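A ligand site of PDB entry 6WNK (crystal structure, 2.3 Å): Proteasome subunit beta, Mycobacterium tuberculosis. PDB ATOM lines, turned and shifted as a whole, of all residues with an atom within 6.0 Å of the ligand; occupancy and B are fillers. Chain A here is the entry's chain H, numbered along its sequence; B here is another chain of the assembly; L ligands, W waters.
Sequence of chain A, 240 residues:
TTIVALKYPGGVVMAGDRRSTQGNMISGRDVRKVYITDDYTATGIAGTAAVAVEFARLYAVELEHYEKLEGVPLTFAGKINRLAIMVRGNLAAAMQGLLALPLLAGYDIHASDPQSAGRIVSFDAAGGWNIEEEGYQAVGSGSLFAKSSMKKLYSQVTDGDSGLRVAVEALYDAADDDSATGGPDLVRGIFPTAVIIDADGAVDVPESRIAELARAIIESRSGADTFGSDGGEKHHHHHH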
ATOM      1  N   THR A   1      14.403  -1.764  28.426  1.00  0.00           N
ATOM      2  CA  THR A   1      13.168  -2.530  28.307  1.00  0.00           C
ATOM      3  C   THR A   1      12.649  -2.956  29.667  1.00  0.00           C
ATOM      4  O   THR A   1      13.421  -3.334  30.546  1.00  0.00           O
ATOM      5  CB  THR A   1      13.357  -3.789  27.437  1.00  0.00           C
ATOM      6  OG1 THR A   1      13.611  -3.403  26.073  1.00  0.00           O
ATOM      7  CG2 THR A   1      12.126  -4.700  27.484  1.00  0.00           C
ATOM      8  N   ARG A  19      10.494   1.676  24.162  1.00  0.00           N
ATOM      9  CA  ARG A  19      11.777   2.308  23.892  1.00  0.00           C
ATOM     10  C   ARG A  19      12.796   1.318  23.357  1.00  0.00           C
ATOM     11  O   ARG A  19      12.907   0.185  23.843  1.00  0.00           O
ATOM     12  CB  ARG A  19      12.324   2.966  25.161  1.00  0.00           C
ATOM     13  CG  ARG A  19      13.776   3.392  25.064  1.00  0.00           C
ATOM     14  CD  ARG A  19      14.128   4.403  26.135  1.00  0.00           C
ATOM     15  NE  ARG A  19      13.338   5.617  25.998  1.00  0.00           N
ATOM     16  CZ  ARG A  19      13.464   6.696  26.765  1.00  0.00           C
ATOM     17  NH1 ARG A  19      14.361   6.711  27.748  1.00  0.00           N
ATOM     18  NH2 ARG A  19      12.697   7.751  26.552  1.00  0.00           N
ATOM     19  N   SER A  20      13.543   1.746  22.340  1.00  0.00           N
ATOM     20  CA  SER A  20      14.788   1.096  21.972  1.00  0.00           C
ATOM     21  C   SER A  20      15.906   2.121  22.068  1.00  0.00           C
ATOM     22  O   SER A  20      15.703   3.302  21.749  1.00  0.00           O
ATOM     23  CB  SER A  20      14.732   0.474  20.573  1.00  0.00           C
ATOM     24  OG  SER A  20      14.777   1.462  19.550  1.00  0.00           O
ATOM     25  N   THR A  21      17.077   1.679  22.514  1.00  0.00           N
ATOM     26  CA  THR A  21      18.243   2.533  22.631  1.00  0.00           C
ATOM     27  C   THR A  21      19.382   1.971  21.799  1.00  0.00           C
ATOM     28  O   THR A  21      19.356   0.809  21.362  1.00  0.00           O
ATOM     29  CB  THR A  21      18.688   2.684  24.098  1.00  0.00           C
ATOM     30  OG1 THR A  21      19.008   1.394  24.635  1.00  0.00           O
ATOM     31  CG2 THR A  21      17.583   3.316  24.929  1.00  0.00           C
ATOM     32  N   GLN A  22      20.383   2.806  21.585  1.00  0.00           N
ATOM     33  CA  GLN A  22      21.632   2.435  20.916  1.00  0.00           C
ATOM     34  C   GLN A  22      22.717   3.193  21.689  1.00  0.00           C
ATOM     35  O   GLN A  22      22.998   4.356  21.403  1.00  0.00           O
ATOM     36  CB  GLN A  22      21.601   2.804  19.433  1.00  0.00           C
ATOM     37  CG  GLN A  22      22.667   2.120  18.592  1.00  0.00           C
ATOM     38  CD  GLN A  22      22.391   2.244  17.102  1.00  0.00           C
ATOM     39  OE1 GLN A  22      23.301   2.538  16.326  1.00  0.00           O
ATOM     40  NE2 GLN A  22      21.155   1.996  16.688  1.00  0.00           N
ATOM     41  N   GLY A  23      23.271   2.531  22.702  1.00  0.00           N
ATOM     42  CA  GLY A  23      24.112   3.240  23.650  1.00  0.00           C
ATOM     43  C   GLY A  23      23.258   4.143  24.531  1.00  0.00           C
ATOM     44  O   GLY A  23      22.224   3.730  25.066  1.00  0.00           O
ATOM     45  N   SER A  27      16.837   5.302  20.053  1.00  0.00           N
ATOM     46  CA  SER A  27      16.712   4.927  18.657  1.00  0.00           C
ATOM     47  C   SER A  27      15.299   4.532  18.261  1.00  0.00           C
ATOM     48  O   SER A  27      15.059   4.307  17.073  1.00  0.00           O
ATOM     49  CB  SER A  27      17.667   3.779  18.315  1.00  0.00           C
ATOM     50  OG  SER A  27      17.339   2.587  19.006  1.00  0.00           O
ATOM     51  N   GLY A  28      14.382   4.415  19.209  1.00  0.00           N
ATOM     52  CA  GLY A  28      13.012   4.030  18.901  1.00  0.00           C
ATOM     53  C   GLY A  28      12.080   4.468  20.003  1.00  0.00           C
ATOM     54  O   GLY A  28      12.457   4.524  21.172  1.00  0.00           O
ATOM     55  N   VAL A  31       8.296   0.959  19.775  1.00  0.00           N
ATOM     56  CA  VAL A  31       8.570  -0.463  19.652  1.00  0.00           C
ATOM     57  C   VAL A  31       7.481  -1.234  20.382  1.00  0.00           C
ATOM     58  O   VAL A  31       7.112  -0.907  21.513  1.00  0.00           O
ATOM     59  CB  VAL A  31       9.966  -0.807  20.208  1.00  0.00           C
ATOM     60  CG1 VAL A  31      10.304  -2.240  19.896  1.00  0.00           C
ATOM     61  CG2 VAL A  31      11.015   0.144  19.652  1.00  0.00           C
ATOM     62  N   ARG A  32       6.962  -2.266  19.727  1.00  0.00           N
ATOM     63  CA  ARG A  32       5.956  -3.147  20.310  1.00  0.00           C
ATOM     64  C   ARG A  32       6.660  -4.430  20.727  1.00  0.00           C
ATOM     65  O   ARG A  32       7.156  -5.183  19.880  1.00  0.00           O
ATOM     66  CB  ARG A  32       4.824  -3.401  19.317  1.00  0.00           C
ATOM     67  CG  ARG A  32       4.035  -2.137  19.010  1.00  0.00           C
ATOM     68  CD  ARG A  32       3.033  -2.298  17.888  1.00  0.00           C
ATOM     69  NE  ARG A  32       2.253  -1.075  17.710  1.00  0.00           N
ATOM     70  CZ  ARG A  32       2.668  -0.020  17.011  1.00  0.00           C
ATOM     71  NH1 ARG A  32       3.846  -0.036  16.412  1.00  0.00           N
ATOM     72  NH2 ARG A  32       1.895   1.054  16.904  1.00  0.00           N
ATOM     73  N   LYS A  33       6.720  -4.672  22.038  1.00  0.00           N
ATOM     74  CA  LYS A  33       7.521  -5.755  22.588  1.00  0.00           C
ATOM     75  C   LYS A  33       6.690  -6.903  23.146  1.00  0.00           C
ATOM     76  O   LYS A  33       7.265  -7.905  23.572  1.00  0.00           O
ATOM     77  CB  LYS A  33       8.444  -5.215  23.685  1.00  0.00           C
ATOM     78  CG  LYS A  33       9.253  -4.000  23.282  1.00  0.00           C
ATOM     79  CD  LYS A  33      10.135  -3.526  24.424  1.00  0.00           C
ATOM     80  CE  LYS A  33      10.844  -2.219  24.072  1.00  0.00           C
ATOM     81  NZ  LYS A  33      11.690  -1.727  25.184  1.00  0.00           N
ATOM     82  N   TYR A  35       3.887  -9.727  22.341  1.00  0.00           N
ATOM     83  CA  TYR A  35       3.336 -10.427  21.181  1.00  0.00           C
ATOM     84  C   TYR A  35       2.240 -11.386  21.611  1.00  0.00           C
ATOM     85  O   TYR A  35       2.413 -12.134  22.587  1.00  0.00           O
ATOM     86  CB  TYR A  35       4.427 -11.215  20.456  1.00  0.00           C
ATOM     87  CG  TYR A  35       5.415 -10.360  19.690  1.00  0.00           C
ATOM     88  CD1 TYR A  35       6.390  -9.623  20.357  1.00  0.00           C
ATOM     89  CD2 TYR A  35       5.387 -10.307  18.304  1.00  0.00           C
ATOM     90  CE1 TYR A  35       7.302  -8.851  19.660  1.00  0.00           C
ATOM     91  CE2 TYR A  35       6.288  -9.532  17.601  1.00  0.00           C
ATOM     92  CZ  TYR A  35       7.240  -8.806  18.287  1.00  0.00           C
ATOM     93  OH  TYR A  35       8.146  -8.039  17.585  1.00  0.00           O
ATOM     94  N   ILE A  45       9.711  -9.826  25.189  1.00  0.00           N
ATOM     95  CA  ILE A  45      11.135 -10.128  25.117  1.00  0.00           C
ATOM     96  C   ILE A  45      11.937  -8.853  25.362  1.00  0.00           C
ATOM     97  O   ILE A  45      11.538  -7.760  24.942  1.00  0.00           O
ATOM     98  CB  ILE A  45      11.524 -10.767  23.761  1.00  0.00           C
ATOM     99  CG1 ILE A  45      10.487 -11.823  23.377  1.00  0.00           C
ATOM    100  CG2 ILE A  45      12.897 -11.418  23.853  1.00  0.00           C
ATOM    101  CD1 ILE A  45      10.990 -12.856  22.387  1.00  0.00           C
ATOM    102  N   ALA A  46      13.058  -9.008  26.057  1.00  0.00           N
ATOM    103  CA  ALA A  46      14.036  -7.957  26.250  1.00  0.00           C
ATOM    104  C   ALA A  46      15.348  -8.398  25.631  1.00  0.00           C
ATOM    105  O   ALA A  46      15.555  -9.584  25.345  1.00  0.00           O
ATOM    106  CB  ALA A  46      14.224  -7.619  27.737  1.00  0.00           C
ATOM    107  N   GLY A  47      16.247  -7.440  25.400  1.00  0.00           N
ATOM    108  CA  GLY A  47      17.578  -7.729  24.928  1.00  0.00           C
ATOM    109  C   GLY A  47      17.860  -7.066  23.586  1.00  0.00           C
ATOM    110  O   GLY A  47      17.324  -6.002  23.278  1.00  0.00           O
ATOM    111  N   THR A  48      18.732  -7.705  22.813  1.00  0.00           N
ATOM    112  CA  THR A  48      19.068  -7.197  21.486  1.00  0.00           C
ATOM    113  C   THR A  48      17.837  -7.213  20.607  1.00  0.00           C
ATOM    114  O   THR A  48      17.172  -8.246  20.456  1.00  0.00           O
ATOM    115  CB  THR A  48      20.189  -8.039  20.876  1.00  0.00           C
ATOM    116  OG1 THR A  48      21.213  -8.259  21.844  1.00  0.00           O
ATOM    117  CG2 THR A  48      20.782  -7.332  19.649  1.00  0.00           C
ATOM    118  N   ALA A  49      17.532  -6.058  20.019  1.00  0.00           N
ATOM    119  CA  ALA A  49      16.275  -5.889  19.290  1.00  0.00           C
ATOM    120  C   ALA A  49      16.117  -6.916  18.179  1.00  0.00           C
ATOM    121  O   ALA A  49      15.058  -7.539  18.029  1.00  0.00           O
ATOM    122  CB  ALA A  49      16.172  -4.476  18.732  1.00  0.00           C
ATOM    123  N   ALA A  50      17.176  -7.113  17.378  1.00  0.00           N
ATOM    124  CA  ALA A  50      17.104  -8.060  16.265  1.00  0.00           C
ATOM    125  C   ALA A  50      16.748  -9.461  16.745  1.00  0.00           C
ATOM    126  O   ALA A  50      15.916 -10.143  16.129  1.00  0.00           O
ATOM    127  CB  ALA A  50      18.442  -8.076  15.515  1.00  0.00           C
ATOM    128  N   ALA A  52      15.388 -10.374  19.756  1.00  0.00           N
ATOM    129  CA  ALA A  52      14.080 -10.396  20.409  1.00  0.00           C
ATOM    130  C   ALA A  52      12.962 -10.503  19.381  1.00  0.00           C
ATOM    131  O   ALA A  52      12.049 -11.320  19.522  1.00  0.00           O
ATOM    132  CB  ALA A  52      13.906  -9.151  21.274  1.00  0.00           C
ATOM    133  N   VAL A  53      13.027  -9.678  18.328  1.00  0.00           N
ATOM    134  CA  VAL A  53      11.986  -9.698  17.304  1.00  0.00           C
ATOM    135  C   VAL A  53      11.961 -11.040  16.585  1.00  0.00           C
ATOM    136  O   VAL A  53      10.892 -11.626  16.352  1.00  0.00           O
ATOM    137  CB  VAL A  53      12.186  -8.529  16.315  1.00  0.00           C
ATOM    138  CG1 VAL A  53      11.323  -8.720  15.083  1.00  0.00           C
ATOM    139  CG2 VAL A  53      11.851  -7.210  16.999  1.00  0.00           C
ATOM    140  N   GLY A  97      26.719 -10.988  22.730  1.00  0.00           N
ATOM    141  CA  GLY A  97      25.939  -9.771  22.694  1.00  0.00           C
ATOM    142  C   GLY A  97      24.655  -9.816  21.896  1.00  0.00           C
ATOM    143  O   GLY A  97      24.046  -8.765  21.695  1.00  0.00           O
ATOM    144  N   SER B 122      14.646   1.420   8.786  1.00  0.00           N
ATOM    145  CA  SER B 122      16.053   1.452   9.146  1.00  0.00           C
ATOM    146  C   SER B 122      16.489   0.093   9.681  1.00  0.00           C
ATOM    147  O   SER B 122      15.676  -0.756  10.056  1.00  0.00           O
ATOM    148  CB  SER B 122      16.330   2.549  10.164  1.00  0.00           C
ATOM    149  OG  SER B 122      15.361   2.562  11.199  1.00  0.00           O
ATOM    150  N   PHE B 123      17.804  -0.120   9.677  1.00  0.00           N
ATOM    151  CA  PHE B 123      18.408  -1.401  10.009  1.00  0.00           C
ATOM    152  C   PHE B 123      19.628  -1.160  10.900  1.00  0.00           C
ATOM    153  O   PHE B 123      20.198  -0.072  10.920  1.00  0.00           O
ATOM    154  CB  PHE B 123      18.814  -2.167   8.747  1.00  0.00           C
ATOM    155  CG  PHE B 123      17.653  -2.562   7.864  1.00  0.00           C
ATOM    156  CD1 PHE B 123      17.037  -1.634   7.042  1.00  0.00           C
ATOM    157  CD2 PHE B 123      17.185  -3.870   7.865  1.00  0.00           C
ATOM    158  CE1 PHE B 123      15.973  -1.998   6.236  1.00  0.00           C
ATOM    159  CE2 PHE B 123      16.120  -4.235   7.059  1.00  0.00           C
ATOM    160  CZ  PHE B 123      15.511  -3.302   6.242  1.00  0.00           C
ATOM    161  N   ASP B 124      20.011  -2.181  11.656  1.00  0.00           N
ATOM    162  CA  ASP B 124      21.261  -2.143  12.408  1.00  0.00           C
ATOM    163  C   ASP B 124      22.138  -3.329  12.011  1.00  0.00           C
ATOM    164  O   ASP B 124      21.726  -4.215  11.258  1.00  0.00           O
ATOM    165  CB  ASP B 124      21.012  -2.093  13.929  1.00  0.00           C
ATOM    166  CG  ASP B 124      20.389  -3.368  14.507  1.00  0.00           C
ATOM    167  OD1 ASP B 124      20.553  -4.472  13.936  1.00  0.00           O
ATOM    168  OD2 ASP B 124      19.731  -3.268  15.571  1.00  0.00           O
ATOM    169  N   ALA B 125      23.364  -3.342  12.536  1.00  0.00           N
ATOM    170  CA  ALA B 125      24.364  -4.320  12.111  1.00  0.00           C
ATOM    171  C   ALA B 125      23.978  -5.751  12.484  1.00  0.00           C
ATOM    172  O   ALA B 125      24.507  -6.685  11.884  1.00  0.00           O
ATOM    173  CB  ALA B 125      25.722  -3.978  12.713  1.00  0.00           C
ATOM    174  N   ALA B 126      23.080  -5.938  13.442  1.00  0.00           N
ATOM    175  CA  ALA B 126      22.640  -7.266  13.837  1.00  0.00           C
ATOM    176  C   ALA B 126      21.476  -7.785  13.012  1.00  0.00           C
ATOM    177  O   ALA B 126      20.922  -8.827  13.331  1.00  0.00           O
ATOM    178  CB  ALA B 126      22.256  -7.275  15.324  1.00  0.00           C
ATOM    179  N   GLY B 128      18.646  -6.147  12.781  1.00  0.00           N
ATOM    180  CA  GLY B 128      17.414  -5.539  13.256  1.00  0.00           C
ATOM    181  C   GLY B 128      16.825  -4.603  12.214  1.00  0.00           C
ATOM    182  O   GLY B 128      17.541  -4.005  11.411  1.00  0.00           O
ATOM    183  N   TRP B 129      15.503  -4.502  12.229  1.00  0.00           N
ATOM    184  CA  TRP B 129      14.789  -3.618  11.326  1.00  0.00           C
ATOM    185  C   TRP B 129      13.659  -2.941  12.102  1.00  0.00           C
ATOM    186  O   TRP B 129      13.056  -3.543  12.997  1.00  0.00           O
ATOM    187  CB  TRP B 129      14.223  -4.365  10.100  1.00  0.00           C
ATOM    188  CG  TRP B 129      13.346  -5.522  10.473  1.00  0.00           C
ATOM    189  CD1 TRP B 129      13.733  -6.815  10.670  1.00  0.00           C
ATOM    190  CD2 TRP B 129      11.927  -5.486  10.701  1.00  0.00           C
ATOM    191  NE1 TRP B 129      12.654  -7.591  11.002  1.00  0.00           N
ATOM    192  CE2 TRP B 129      11.535  -6.796  11.034  1.00  0.00           C
ATOM    193  CE3 TRP B 129      10.965  -4.472  10.669  1.00  0.00           C
ATOM    194  CZ2 TRP B 129      10.206  -7.127  11.320  1.00  0.00           C
ATOM    195  CZ3 TRP B 129       9.647  -4.805  10.961  1.00  0.00           C
ATOM    196  CH2 TRP B 129       9.283  -6.113  11.276  1.00  0.00           C
ATOM    197  N   ASN B 130      13.388  -1.692  11.742  1.00  0.00           N
ATOM    198  CA  ASN B 130      12.340  -0.916  12.385  1.00  0.00           C
ATOM    199  C   ASN B 130      11.644  -0.067  11.321  1.00  0.00           C
ATOM    200  O   ASN B 130      12.292   0.728  10.632  1.00  0.00           O
ATOM    201  CB  ASN B 130      12.912  -0.032  13.498  1.00  0.00           C
ATOM    202  CG  ASN B 130      11.827   0.627  14.334  1.00  0.00           C
ATOM    203  OD1 ASN B 130      10.831  -0.004  14.697  1.00  0.00           O
ATOM    204  ND2 ASN B 130      12.007   1.909  14.638  1.00  0.00           N
HETATM  205  C1  LIG L   1      22.012  -1.667  18.095  1.00  0.00           C
HETATM  206  O1  LIG L   1      22.358  -1.049  19.042  1.00  0.00           O
HETATM  207  C2  LIG L   1      23.015  -2.166  17.061  1.00  0.00           C
HETATM  208  C3  LIG L   1      23.288  -3.671  17.183  1.00  0.00           C
HETATM  209  C4  LIG L   1      24.327  -3.853  18.286  1.00  0.00           C
HETATM  210  C5  LIG L   1      23.928  -4.258  19.546  1.00  0.00           C
HETATM  211  C6  LIG L   1      24.864  -4.403  20.570  1.00  0.00           C
HETATM  212  C7  LIG L   1      26.208  -4.144  20.303  1.00  0.00           C
HETATM  213  C8  LIG L   1      26.606  -3.729  19.033  1.00  0.00           C
HETATM  214  C9  LIG L   1      25.667  -3.582  18.032  1.00  0.00           C
HETATM  215  C10 LIG L   1      16.970  -1.406  13.725  1.00  0.00           C
HETATM  216  C11 LIG L   1      15.677  -1.748  15.909  1.00  0.00           C
HETATM  217  C12 LIG L   1      13.735  -3.141  16.141  1.00  0.00           C
HETATM  218  C13 LIG L   1      15.081  -0.772  16.689  1.00  0.00           C
HETATM  219  C14 LIG L   1      19.278  -2.533  19.936  1.00  0.00           C
HETATM  220  C15 LIG L   1      19.607  -1.533  18.841  1.00  0.00           C
HETATM  221  C16 LIG L   1      18.315  -1.366  18.043  1.00  0.00           C
HETATM  222  C17 LIG L   1      18.292  -0.224  17.042  1.00  0.00           C
HETATM  223  C18 LIG L   1      17.534   0.714  14.578  1.00  0.00           C
HETATM  224  C19 LIG L   1      16.973   0.128  13.468  1.00  0.00           C
HETATM  225  C20 LIG L   1      17.081  -1.541  15.325  1.00  0.00           C
HETATM  226  C21 LIG L   1      15.007  -2.932  15.631  1.00  0.00           C
HETATM  227  C22 LIG L   1      13.139  -2.165  16.922  1.00  0.00           C
HETATM  228  C23 LIG L   1      13.815  -0.989  17.201  1.00  0.00           C
HETATM  229  N1  LIG L   1      17.656  -0.423  15.758  1.00  0.00           N
HETATM  230  N2  LIG L   1      20.600  -1.982  17.905  1.00  0.00           N
HETATM  231  O2  LIG L   1      19.319  -3.710  19.740  1.00  0.00           O
HETATM  232  O3  LIG L   1      18.774   0.819  17.344  1.00  0.00           O
HETATM  233  N3  LIG L   1      18.875  -1.991  21.217  1.00  0.00           N
HETATM  234  C24 LIG L   1      18.500  -2.837  22.326  1.00  0.00           C
HETATM  235  C25 LIG L   1      17.079  -2.427  22.670  1.00  0.00           C
HETATM  236  O4  LIG L   1      16.796  -1.270  22.774  1.00  0.00           O
HETATM  237  C26 LIG L   1      19.474  -2.648  23.495  1.00  0.00           C
HETATM  238  C27 LIG L   1      20.829  -3.214  23.068  1.00  0.00           C
HETATM  239  C28 LIG L   1      21.063  -4.578  23.170  1.00  0.00           C
HETATM  240  C29 LIG L   1      21.793  -2.369  22.560  1.00  0.00           C
HETATM  241  C30 LIG L   1      22.280  -5.095  22.774  1.00  0.00           C
HETATM  242  C31 LIG L   1      23.016  -2.880  22.170  1.00  0.00           C
HETATM  243  C32 LIG L   1      23.261  -4.251  22.264  1.00  0.00           C
HETATM  244  O5  LIG L   1      24.491  -4.809  21.857  1.00  0.00           O
HETATM  245  C33 LIG L   1      14.702  -3.094  23.152  1.00  0.00           C
HETATM  246  C34 LIG L   1      13.542  -3.754  21.007  1.00  0.00           C
HETATM  247  C35 LIG L   1      12.727  -4.597  20.264  1.00  0.00           C
HETATM  248  C36 LIG L   1      13.794  -4.022  22.348  1.00  0.00           C
HETATM  249  C37 LIG L   1      12.169  -5.716  20.864  1.00  0.00           C
HETATM  250  C38 LIG L   1      12.432  -5.991  22.199  1.00  0.00           C
HETATM  251  C39 LIG L   1      13.247  -5.148  22.941  1.00  0.00           C
HETATM  252  F1  LIG L   1      14.089  -2.648  20.434  1.00  0.00           F
HETATM  253  N4  LIG L   1      16.073  -3.442  22.848  1.00  0.00           N
HETATM  254  O   HOH W   1      21.919   0.093  24.717  1.00  0.00           O
HETATM  255  O   HOH W   2      19.518  -5.236  17.460  1.00  0.00           O
HETATM  256  O   HOH W   3      24.666  -0.196  20.348  1.00  0.00           O
HETATM  257  O   HOH W   4      16.389   0.160  25.348  1.00  0.00           O
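The side-chain amide nitrogen (NE2) of Gln 22 is in hydrogen-bond range of an oxygen (O3) of the ligand.
N2 of the ligand sits at hydrogen-bond distance from OD2 of Asp 124 of chain B (2.8 Å).
O3 of the ligand sits at hydrogen-bond distance from OG of Ser 27 (2.8 Å).
O4 of the ligand lies within hydrogen-bond range of N of Thr 21 (3.0 Å).
The backbone carbonyl oxygen (O) of Thr 21 is in hydrogen-bond range of a nitrogen (N3) of the ligand (2.8 Å).
O of Gly 47 lies within hydrogen-bond range of N4 of the ligand (2.9 Å).
The backbone NH (N) of Ala 49 lies within hydrogen-bond range of an oxygen (O2) of the ligand.
The side-chain carboxylate of Asp 124 of chain B is in hydrogen-bond range of the backbone NH of Gly 128 of chain B (2.8 Å).
N of Ala 126 of chain B lies within hydrogen-bond range of OD1 of Asp 124 of chain B, 3.0 Å away.
The side-chain hydroxyl (OG) of Ser 27 sits at hydrogen-bond distance from the side-chain hydroxyl (OG) of Ser 20 (2.9 Å).
OG1 of Thr 1 is in hydrogen-bond range of NZ of Lys 33 (2.7 Å).
The side-chain hydroxyl (OG) of Ser 20 sits at hydrogen-bond distance from the backbone NH (N) of Gly 28, at 3.0 Å.
OG1 of Thr 48 lies within hydrogen-bond range of O of Gly 97 (2.9 Å).
N of Asn 130 of chain B lies within hydrogen-bond range of O of Ser 122 of chain B, 3.0 Å away.
The side-chain amino group (NZ) of Lys 33 sits at hydrogen-bond distance from the backbone carbonyl oxygen (O) of Arg 19 (2.6 Å).
Residues that only touch the ligand: Thr 1, Arg 19, Ser 20, Val 31, Lys 33, Ile 45, Thr 48, Ala 52, Gly 97, Ser 122 of chain B, Phe 123 of chain B, Gly 128 of chain B, Trp 129 of chain B and Asn 130 of chain B.
Of the 29 residues printed, 20 come within 4 Å of the ligand.
Water W2 lies within hydrogen-bond range of OD2 of Asp 124 of chain B, O2 of the ligand, N of Ala 50 and N of Ala 49.
Water W4 lies within hydrogen-bond range of an oxygen (O4) of the ligand (3.0 Å) and the side-chain hydroxyl (OG1) of Thr 21 (3.0 Å).
Water W1 bridges OG1 of Thr 21 (3.2 Å) and N of Gly 23 (3.4 Å).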
